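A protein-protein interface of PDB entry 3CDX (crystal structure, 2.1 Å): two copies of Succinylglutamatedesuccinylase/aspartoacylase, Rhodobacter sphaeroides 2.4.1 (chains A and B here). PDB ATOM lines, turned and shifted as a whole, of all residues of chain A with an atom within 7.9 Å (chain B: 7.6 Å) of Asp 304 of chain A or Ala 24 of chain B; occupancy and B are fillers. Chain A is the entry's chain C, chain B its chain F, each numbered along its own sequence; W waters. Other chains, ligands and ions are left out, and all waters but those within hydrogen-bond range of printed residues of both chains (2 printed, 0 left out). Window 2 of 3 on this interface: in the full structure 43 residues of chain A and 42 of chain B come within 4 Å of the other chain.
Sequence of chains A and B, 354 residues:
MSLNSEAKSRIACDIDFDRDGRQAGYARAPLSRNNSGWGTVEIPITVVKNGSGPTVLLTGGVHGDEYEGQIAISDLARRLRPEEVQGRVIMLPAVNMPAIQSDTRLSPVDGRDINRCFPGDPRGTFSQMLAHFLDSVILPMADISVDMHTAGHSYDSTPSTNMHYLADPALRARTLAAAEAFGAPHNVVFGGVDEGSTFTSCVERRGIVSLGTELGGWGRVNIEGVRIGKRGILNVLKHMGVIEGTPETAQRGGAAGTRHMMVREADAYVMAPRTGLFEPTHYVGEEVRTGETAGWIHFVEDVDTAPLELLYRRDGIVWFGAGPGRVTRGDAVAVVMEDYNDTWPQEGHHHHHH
O of Glu 301 of chain A touches CE1 of Tyr 26 of chain B, 3.1 Å away. Tyr 26 of chain B touches Asp 302 of chain A. Val 303 of chain A touches Ala 24 of chain B (CG2 to C, 3.9 Å). Gly 25 of chain B touches Val 303 of chain A. CG1 of Val 303 of chain A touches CB of Pro 44 of chain B, at 3.8 Å. OG1 of Thr 46 of chain B touches CG1 of Val 303 of chain A, at 3.9 Å. Ala 24 of chain B touches Asp 304 of chain A. Asp 304 of chain A touches Arg 78 of chain B. CA of Ala 306 of chain A touches CD of Arg 78 of chain B, 3.6 Å away. Pro 307 of chain A touches Arg 78 of chain B (CD to NH2, 3.8 Å).
Water W1 lies within hydrogen-bond range of the backbone NH (N) of Asp 304 of chain A (2.9 Å), the guanidinium group (NH2) of Arg 22 of chain B (3.2 Å) and the side-chain hydroxyl (OG1) of Thr 46 of chain B (3.3 Å). Water W2 bridges O of Arg 78 of chain B (2.9 Å) and OD1 of Asp 304 of chain A (3.1 Å).
The side-chain hydroxyl of Tyr 26 of chain B lies within hydrogen-bond range of the backbone NH of Val 303 of chain A (3.0 Å). The side-chain carboxylate (OD1) of Asp 304 of chain A lies within salt-bridge range of the guanidinium group (NH2) of Arg 22 of chain B, at 3.0 Å.
The side-chain hydroxyl (OG1) of Thr 305 of chain A sits at hydrogen-bond distance from the side-chain carboxylate (OD2) of Asp 302 of chain A (2.7 Å). The side-chain hydroxyl of Thr 305 of chain A sits at hydrogen-bond distance from the backbone carbonyl oxygen of Val 303 of chain A (3.4 Å). NH2 of Arg 22 of chain B lies within hydrogen-bond range of O of Ala 77 of chain B (2.9 Å). The backbone NH (N) of Ile 45 of chain B lies within hydrogen-bond range of the backbone carbonyl oxygen (O) of Gly 25 of chain B (2.9 Å).
Printed residues of chain B within 4 Å of Glu 301 of chain A: Tyr 26 (3.1 Å). Of the printed residues of chain B, Asp 302 of chain A touches Tyr 26. Of chain B, only Arg 22, Ala 24 and Arg 78 come within 4 Å of Asp 304 of chain A. Of the printed residues of chain B, Ala 306 of chain A touches Arg 78 (3.6 Å). Of the printed residues of chain A, Arg 22 of chain B touches Asp 304 (3.0 Å). Printed residues of chain A within 4 Å of Ala 24 of chain B: Val 303 and Asp 304. Of the printed residues of chain A, Pro 44 of chain B touches Val 303 (3.8 Å). The nearest residue of chain B that does not touch Asp 304 of chain A is Ala 77 of chain B (5.5 Å). The nearest residue of chain A that does not touch Ala 24 of chain B is Asp 302 of chain A (7.6 Å).
Of the 8 printed residues of chain A, 7 touch a printed residue of chain B. Hydrophobic or aromatic side chains of chain A that line the printed part of chain B: Val 303, Ala 306 and Pro 307. Of the 15 printed residues of chain B, 8 touch a printed residue of chain A. Hydrophobic or aromatic side chains of chain B that line the printed part of chain A: Ala 24, Tyr 26 and Pro 44. Among the printed residues, 14 pairs touch across the chains. Among the printed residues, Asp or Glu carboxylates within 4 Å of a Lys or Arg side-chain nitrogen of the other chain: Asp 304 of chain A with Arg 22 of chain B (3.0 Å).
No position is printed for both chains. Of the 14 pairs that touch across the chains among the printed residues, none has its exchanged pair printed and touching as well.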
ATOM      1  N   PHE A 299       4.952  28.044  -4.253  1.00  0.00           N
ATOM      2  CA  PHE A 299       5.587  29.270  -3.770  1.00  0.00           C
ATOM      3  C   PHE A 299       6.591  29.804  -4.792  1.00  0.00           C
ATOM      4  O   PHE A 299       7.814  29.714  -4.601  1.00  0.00           O
ATOM      5  CB  PHE A 299       6.243  29.013  -2.408  1.00  0.00           C
ATOM      6  CG  PHE A 299       5.289  28.442  -1.427  1.00  0.00           C
ATOM      7  CD1 PHE A 299       4.368  29.273  -0.776  1.00  0.00           C
ATOM      8  CD2 PHE A 299       5.218  27.065  -1.230  1.00  0.00           C
ATOM      9  CE1 PHE A 299       3.411  28.726   0.102  1.00  0.00           C
ATOM     10  CE2 PHE A 299       4.276  26.511  -0.368  1.00  0.00           C
ATOM     11  CZ  PHE A 299       3.375  27.354   0.313  1.00  0.00           C
ATOM     12  N   GLU A 301       7.599  32.617  -5.649  1.00  0.00           N
ATOM     13  CA  GLU A 301       8.579  33.607  -5.189  1.00  0.00           C
ATOM     14  C   GLU A 301       9.936  32.952  -4.736  1.00  0.00           C
ATOM     15  O   GLU A 301      10.969  33.622  -4.672  1.00  0.00           O
ATOM     16  CB  GLU A 301       7.969  34.447  -4.050  1.00  0.00           C
ATOM     17  CG  GLU A 301       7.641  33.658  -2.782  1.00  0.00           C
ATOM     18  CD  GLU A 301       6.246  33.022  -2.797  1.00  0.00           C
ATOM     19  OE1 GLU A 301       5.741  32.705  -1.695  1.00  0.00           O
ATOM     20  OE2 GLU A 301       5.636  32.861  -3.888  1.00  0.00           O
ATOM     21  N   ASP A 302       9.899  31.650  -4.429  1.00  0.00           N
ATOM     22  CA  ASP A 302      11.064  30.882  -3.927  1.00  0.00           C
ATOM     23  C   ASP A 302      11.694  30.034  -5.017  1.00  0.00           C
ATOM     24  O   ASP A 302      10.983  29.320  -5.715  1.00  0.00           O
ATOM     25  CB  ASP A 302      10.610  29.875  -2.871  1.00  0.00           C
ATOM     26  CG  ASP A 302      10.402  30.477  -1.516  1.00  0.00           C
ATOM     27  OD1 ASP A 302      10.668  31.691  -1.311  1.00  0.00           O
ATOM     28  OD2 ASP A 302       9.952  29.718  -0.621  1.00  0.00           O
ATOM     29  N   VAL A 303      13.021  30.048  -5.133  1.00  0.00           N
ATOM     30  CA  VAL A 303      13.652  28.951  -5.850  1.00  0.00           C
ATOM     31  C   VAL A 303      13.621  27.738  -4.875  1.00  0.00           C
ATOM     32  O   VAL A 303      13.361  27.913  -3.684  1.00  0.00           O
ATOM     33  CB  VAL A 303      15.091  29.261  -6.362  1.00  0.00           C
ATOM     34  CG1 VAL A 303      15.095  30.341  -7.440  1.00  0.00           C
ATOM     35  CG2 VAL A 303      16.094  29.591  -5.191  1.00  0.00           C
ATOM     36  N   ASP A 304      13.846  26.530  -5.397  1.00  0.00           N
ATOM     37  CA  ASP A 304      14.040  25.308  -4.585  1.00  0.00           C
ATOM     38  C   ASP A 304      12.763  24.819  -3.855  1.00  0.00           C
ATOM     39  O   ASP A 304      12.478  23.638  -3.890  1.00  0.00           O
ATOM     40  CB  ASP A 304      15.260  25.447  -3.625  1.00  0.00           C
ATOM     41  CG  ASP A 304      16.640  25.422  -4.370  1.00  0.00           C
ATOM     42  OD1 ASP A 304      16.770  24.723  -5.400  1.00  0.00           O
ATOM     43  OD2 ASP A 304      17.616  26.065  -3.915  1.00  0.00           O
ATOM     44  N   THR A 305      11.970  25.709  -3.257  1.00  0.00           N
ATOM     45  CA  THR A 305      10.819  25.325  -2.388  1.00  0.00           C
ATOM     46  C   THR A 305       9.743  24.455  -3.053  1.00  0.00           C
ATOM     47  O   THR A 305       9.122  24.862  -4.058  1.00  0.00           O
ATOM     48  CB  THR A 305      10.160  26.584  -1.757  1.00  0.00           C
ATOM     49  OG1 THR A 305      11.158  27.377  -1.093  1.00  0.00           O
ATOM     50  CG2 THR A 305       9.081  26.221  -0.744  1.00  0.00           C
ATOM     51  N   ALA A 306       9.485  23.268  -2.485  1.00  0.00           N
ATOM     52  CA  ALA A 306       8.430  22.394  -3.023  1.00  0.00           C
ATOM     53  C   ALA A 306       7.028  22.906  -2.689  1.00  0.00           C
ATOM     54  O   ALA A 306       6.843  23.516  -1.656  1.00  0.00           O
ATOM     55  CB  ALA A 306       8.589  20.978  -2.519  1.00  0.00           C
ATOM     56  N   PRO A 307       6.036  22.636  -3.563  1.00  0.00           N
ATOM     57  CA  PRO A 307       4.668  23.045  -3.261  1.00  0.00           C
ATOM     58  C   PRO A 307       4.058  22.297  -2.073  1.00  0.00           C
ATOM     59  O   PRO A 307       4.489  21.195  -1.728  1.00  0.00           O
ATOM     60  CB  PRO A 307       3.890  22.715  -4.557  1.00  0.00           C
ATOM     61  CG  PRO A 307       4.763  21.828  -5.359  1.00  0.00           C
ATOM     62  CD  PRO A 307       6.154  21.937  -4.868  1.00  0.00           C
ATOM     63  N   ILE B  15      24.699  35.154 -10.304  1.00  0.00           N
ATOM     64  CA  ILE B  15      24.794  33.921 -11.080  1.00  0.00           C
ATOM     65  C   ILE B  15      25.860  34.023 -12.179  1.00  0.00           C
ATOM     66  O   ILE B  15      25.918  35.011 -12.916  1.00  0.00           O
ATOM     67  CB  ILE B  15      23.415  33.544 -11.720  1.00  0.00           C
ATOM     68  CG1 ILE B  15      22.379  33.210 -10.629  1.00  0.00           C
ATOM     69  CG2 ILE B  15      23.582  32.418 -12.740  1.00  0.00           C
ATOM     70  CD1 ILE B  15      21.137  32.440 -11.120  1.00  0.00           C
ATOM     71  N   ARG B  22      24.528  23.604 -11.290  1.00  0.00           N
ATOM     72  CA  ARG B  22      23.246  24.246 -11.018  1.00  0.00           C
ATOM     73  C   ARG B  22      23.403  25.451 -10.082  1.00  0.00           C
ATOM     74  O   ARG B  22      24.087  25.378  -9.061  1.00  0.00           O
ATOM     75  CB  ARG B  22      22.258  23.240 -10.429  1.00  0.00           C
ATOM     76  CG  ARG B  22      20.896  23.836 -10.065  1.00  0.00           C
ATOM     77  CD  ARG B  22      19.876  22.714  -9.819  1.00  0.00           C
ATOM     78  NE  ARG B  22      18.527  23.238  -9.606  1.00  0.00           N
ATOM     79  CZ  ARG B  22      18.085  23.749  -8.460  1.00  0.00           C
ATOM     80  NH1 ARG B  22      18.884  23.814  -7.397  1.00  0.00           N
ATOM     81  NH2 ARG B  22      16.835  24.192  -8.363  1.00  0.00           N
ATOM     82  N   GLN B  23      22.773  26.566 -10.457  1.00  0.00           N
ATOM     83  CA  GLN B  23      22.683  27.723  -9.588  1.00  0.00           C
ATOM     84  C   GLN B  23      21.204  28.144  -9.538  1.00  0.00           C
ATOM     85  O   GLN B  23      20.594  28.357 -10.570  1.00  0.00           O
ATOM     86  CB  GLN B  23      23.579  28.876 -10.105  1.00  0.00           C
ATOM     87  CG  GLN B  23      25.102  28.516 -10.232  1.00  0.00           C
ATOM     88  CD  GLN B  23      25.823  29.457 -11.145  1.00  0.00           C
ATOM     89  OE1 GLN B  23      26.254  30.535 -10.714  1.00  0.00           O
ATOM     90  NE2 GLN B  23      25.948  29.082 -12.430  1.00  0.00           N
ATOM     91  N   ALA B  24      20.645  28.231  -8.340  1.00  0.00           N
ATOM     92  CA  ALA B  24      19.294  28.690  -8.136  1.00  0.00           C
ATOM     93  C   ALA B  24      19.437  29.805  -7.128  1.00  0.00           C
ATOM     94  O   ALA B  24      19.887  29.592  -5.998  1.00  0.00           O
ATOM     95  CB  ALA B  24      18.423  27.573  -7.572  1.00  0.00           C
ATOM     96  N   GLY B  25      19.089  31.000  -7.569  1.00  0.00           N
ATOM     97  CA  GLY B  25      19.155  32.195  -6.754  1.00  0.00           C
ATOM     98  C   GLY B  25      18.169  33.200  -7.336  1.00  0.00           C
ATOM     99  O   GLY B  25      17.164  32.814  -7.946  1.00  0.00           O
ATOM    100  N   TYR B  26      18.462  34.483  -7.149  1.00  0.00           N
ATOM    101  CA  TYR B  26      17.534  35.558  -7.525  1.00  0.00           C
ATOM    102  C   TYR B  26      18.269  36.709  -8.231  1.00  0.00           C
ATOM    103  O   TYR B  26      19.437  36.989  -7.923  1.00  0.00           O
ATOM    104  CB  TYR B  26      16.838  36.096  -6.275  1.00  0.00           C
ATOM    105  CG  TYR B  26      16.097  35.043  -5.472  1.00  0.00           C
ATOM    106  CD1 TYR B  26      14.770  34.711  -5.756  1.00  0.00           C
ATOM    107  CD2 TYR B  26      16.733  34.358  -4.441  1.00  0.00           C
ATOM    108  CE1 TYR B  26      14.091  33.703  -5.019  1.00  0.00           C
ATOM    109  CE2 TYR B  26      16.070  33.364  -3.697  1.00  0.00           C
ATOM    110  CZ  TYR B  26      14.762  33.031  -3.996  1.00  0.00           C
ATOM    111  OH  TYR B  26      14.128  32.043  -3.225  1.00  0.00           O
ATOM    112  N   PRO B  44      13.188  35.034  -9.076  1.00  0.00           N
ATOM    113  CA  PRO B  44      13.779  33.694  -9.130  1.00  0.00           C
ATOM    114  C   PRO B  44      14.436  33.442 -10.475  1.00  0.00           C
ATOM    115  O   PRO B  44      13.810  33.689 -11.517  1.00  0.00           O
ATOM    116  CB  PRO B  44      12.581  32.739  -8.974  1.00  0.00           C
ATOM    117  CG  PRO B  44      11.404  33.554  -8.720  1.00  0.00           C
ATOM    118  CD  PRO B  44      11.755  35.010  -8.724  1.00  0.00           C
ATOM    119  N   ILE B  45      15.681  32.953 -10.433  1.00  0.00           N
ATOM    120  CA  ILE B  45      16.387  32.428 -11.613  1.00  0.00           C
ATOM    121  C   ILE B  45      17.087  31.102 -11.235  1.00  0.00           C
ATOM    122  O   ILE B  45      17.745  31.012 -10.180  1.00  0.00           O
ATOM    123  CB  ILE B  45      17.467  33.384 -12.093  1.00  0.00           C
ATOM    124  CG1 ILE B  45      16.897  34.801 -12.296  1.00  0.00           C
ATOM    125  CG2 ILE B  45      18.087  32.862 -13.403  1.00  0.00           C
ATOM    126  CD1 ILE B  45      17.837  35.771 -13.120  1.00  0.00           C
ATOM    127  N   THR B  46      16.931  30.087 -12.089  1.00  0.00           N
ATOM    128  CA  THR B  46      17.651  28.803 -11.959  1.00  0.00           C
ATOM    129  C   THR B  46      18.304  28.560 -13.303  1.00  0.00           C
ATOM    130  O   THR B  46      17.654  28.694 -14.333  1.00  0.00           O
ATOM    131  CB  THR B  46      16.699  27.623 -11.620  1.00  0.00           C
ATOM    132  OG1 THR B  46      15.992  27.921 -10.418  1.00  0.00           O
ATOM    133  CG2 THR B  46      17.471  26.273 -11.429  1.00  0.00           C
ATOM    134  N   VAL B  47      19.601  28.268 -13.294  1.00  0.00           N
ATOM    135  CA  VAL B  47      20.301  27.870 -14.502  1.00  0.00           C
ATOM    136  C   VAL B  47      20.923  26.494 -14.282  1.00  0.00           C
ATOM    137  O   VAL B  47      21.503  26.209 -13.220  1.00  0.00           O
ATOM    138  CB  VAL B  47      21.452  28.848 -14.887  1.00  0.00           C
ATOM    139  CG1 VAL B  47      22.079  28.426 -16.201  1.00  0.00           C
ATOM    140  CG2 VAL B  47      20.936  30.276 -14.989  1.00  0.00           C
ATOM    141  N   VAL B  48      20.801  25.654 -15.296  1.00  0.00           N
ATOM    142  CA  VAL B  48      21.506  24.391 -15.320  1.00  0.00           C
ATOM    143  C   VAL B  48      22.325  24.364 -16.609  1.00  0.00           C
ATOM    144  O   VAL B  48      21.783  24.609 -17.691  1.00  0.00           O
ATOM    145  CB  VAL B  48      20.530  23.194 -15.271  1.00  0.00           C
ATOM    146  CG1 VAL B  48      21.286  21.902 -15.458  1.00  0.00           C
ATOM    147  CG2 VAL B  48      19.834  23.161 -13.921  1.00  0.00           C
ATOM    148  N   SER B  74       8.622  26.695 -12.619  1.00  0.00           N
ATOM    149  CA  SER B  74       9.137  26.575 -11.275  1.00  0.00           C
ATOM    150  C   SER B  74       9.220  25.096 -10.884  1.00  0.00           C
ATOM    151  O   SER B  74      10.173  24.697 -10.232  1.00  0.00           O
ATOM    152  CB  SER B  74       8.313  27.378 -10.257  1.00  0.00           C
ATOM    153  OG  SER B  74       7.025  26.809 -10.059  1.00  0.00           O
ATOM    154  N   ALA B  77      12.247  23.809 -12.622  1.00  0.00           N
ATOM    155  CA  ALA B  77      13.441  24.410 -12.057  1.00  0.00           C
ATOM    156  C   ALA B  77      13.862  23.663 -10.804  1.00  0.00           C
ATOM    157  O   ALA B  77      15.039  23.526 -10.521  1.00  0.00           O
ATOM    158  CB  ALA B  77      13.212  25.885 -11.728  1.00  0.00           C
ATOM    159  N   ARG B  78      12.889  23.188 -10.054  1.00  0.00           N
ATOM    160  CA  ARG B  78      13.167  22.529  -8.812  1.00  0.00           C
ATOM    161  C   ARG B  78      13.757  21.149  -9.094  1.00  0.00           C
ATOM    162  O   ARG B  78      14.591  20.670  -8.338  1.00  0.00           O
ATOM    163  CB  ARG B  78      11.876  22.434  -8.004  1.00  0.00           C
ATOM    164  CG  ARG B  78      11.977  21.763  -6.667  1.00  0.00           C
ATOM    165  CD  ARG B  78      10.688  21.945  -5.836  1.00  0.00           C
ATOM    166  NE  ARG B  78       9.531  21.294  -6.442  1.00  0.00           N
ATOM    167  CZ  ARG B  78       9.238  19.989  -6.349  1.00  0.00           C
ATOM    168  NH1 ARG B  78      10.039  19.151  -5.678  1.00  0.00           N
ATOM    169  NH2 ARG B  78       8.140  19.518  -6.937  1.00  0.00           N
ATOM    170  N   ARG B  79      13.365  20.546 -10.211  1.00  0.00           N
ATOM    171  CA  ARG B  79      13.625  19.133 -10.422  1.00  0.00           C
ATOM    172  C   ARG B  79      14.728  18.803 -11.419  1.00  0.00           C
ATOM    173  O   ARG B  79      15.292  17.700 -11.369  1.00  0.00           O
ATOM    174  CB  ARG B  79      12.335  18.408 -10.809  1.00  0.00           C
ATOM    175  CG  ARG B  79      11.300  18.418  -9.678  1.00  0.00           C
ATOM    176  CD  ARG B  79      10.102  17.513  -9.945  1.00  0.00           C
ATOM    177  NE  ARG B  79       9.341  17.971 -11.095  1.00  0.00           N
ATOM    178  CZ  ARG B  79       9.453  17.488 -12.330  1.00  0.00           C
ATOM    179  NH1 ARG B  79      10.300  16.487 -12.590  1.00  0.00           N
ATOM    180  NH2 ARG B  79       8.711  18.014 -13.318  1.00  0.00           N
HETATM  181  O   HOH W   1      14.361  26.170  -8.214  1.00  0.00           O
HETATM  182  O   HOH W   2      15.750  21.798  -5.880  1.00  0.00           O
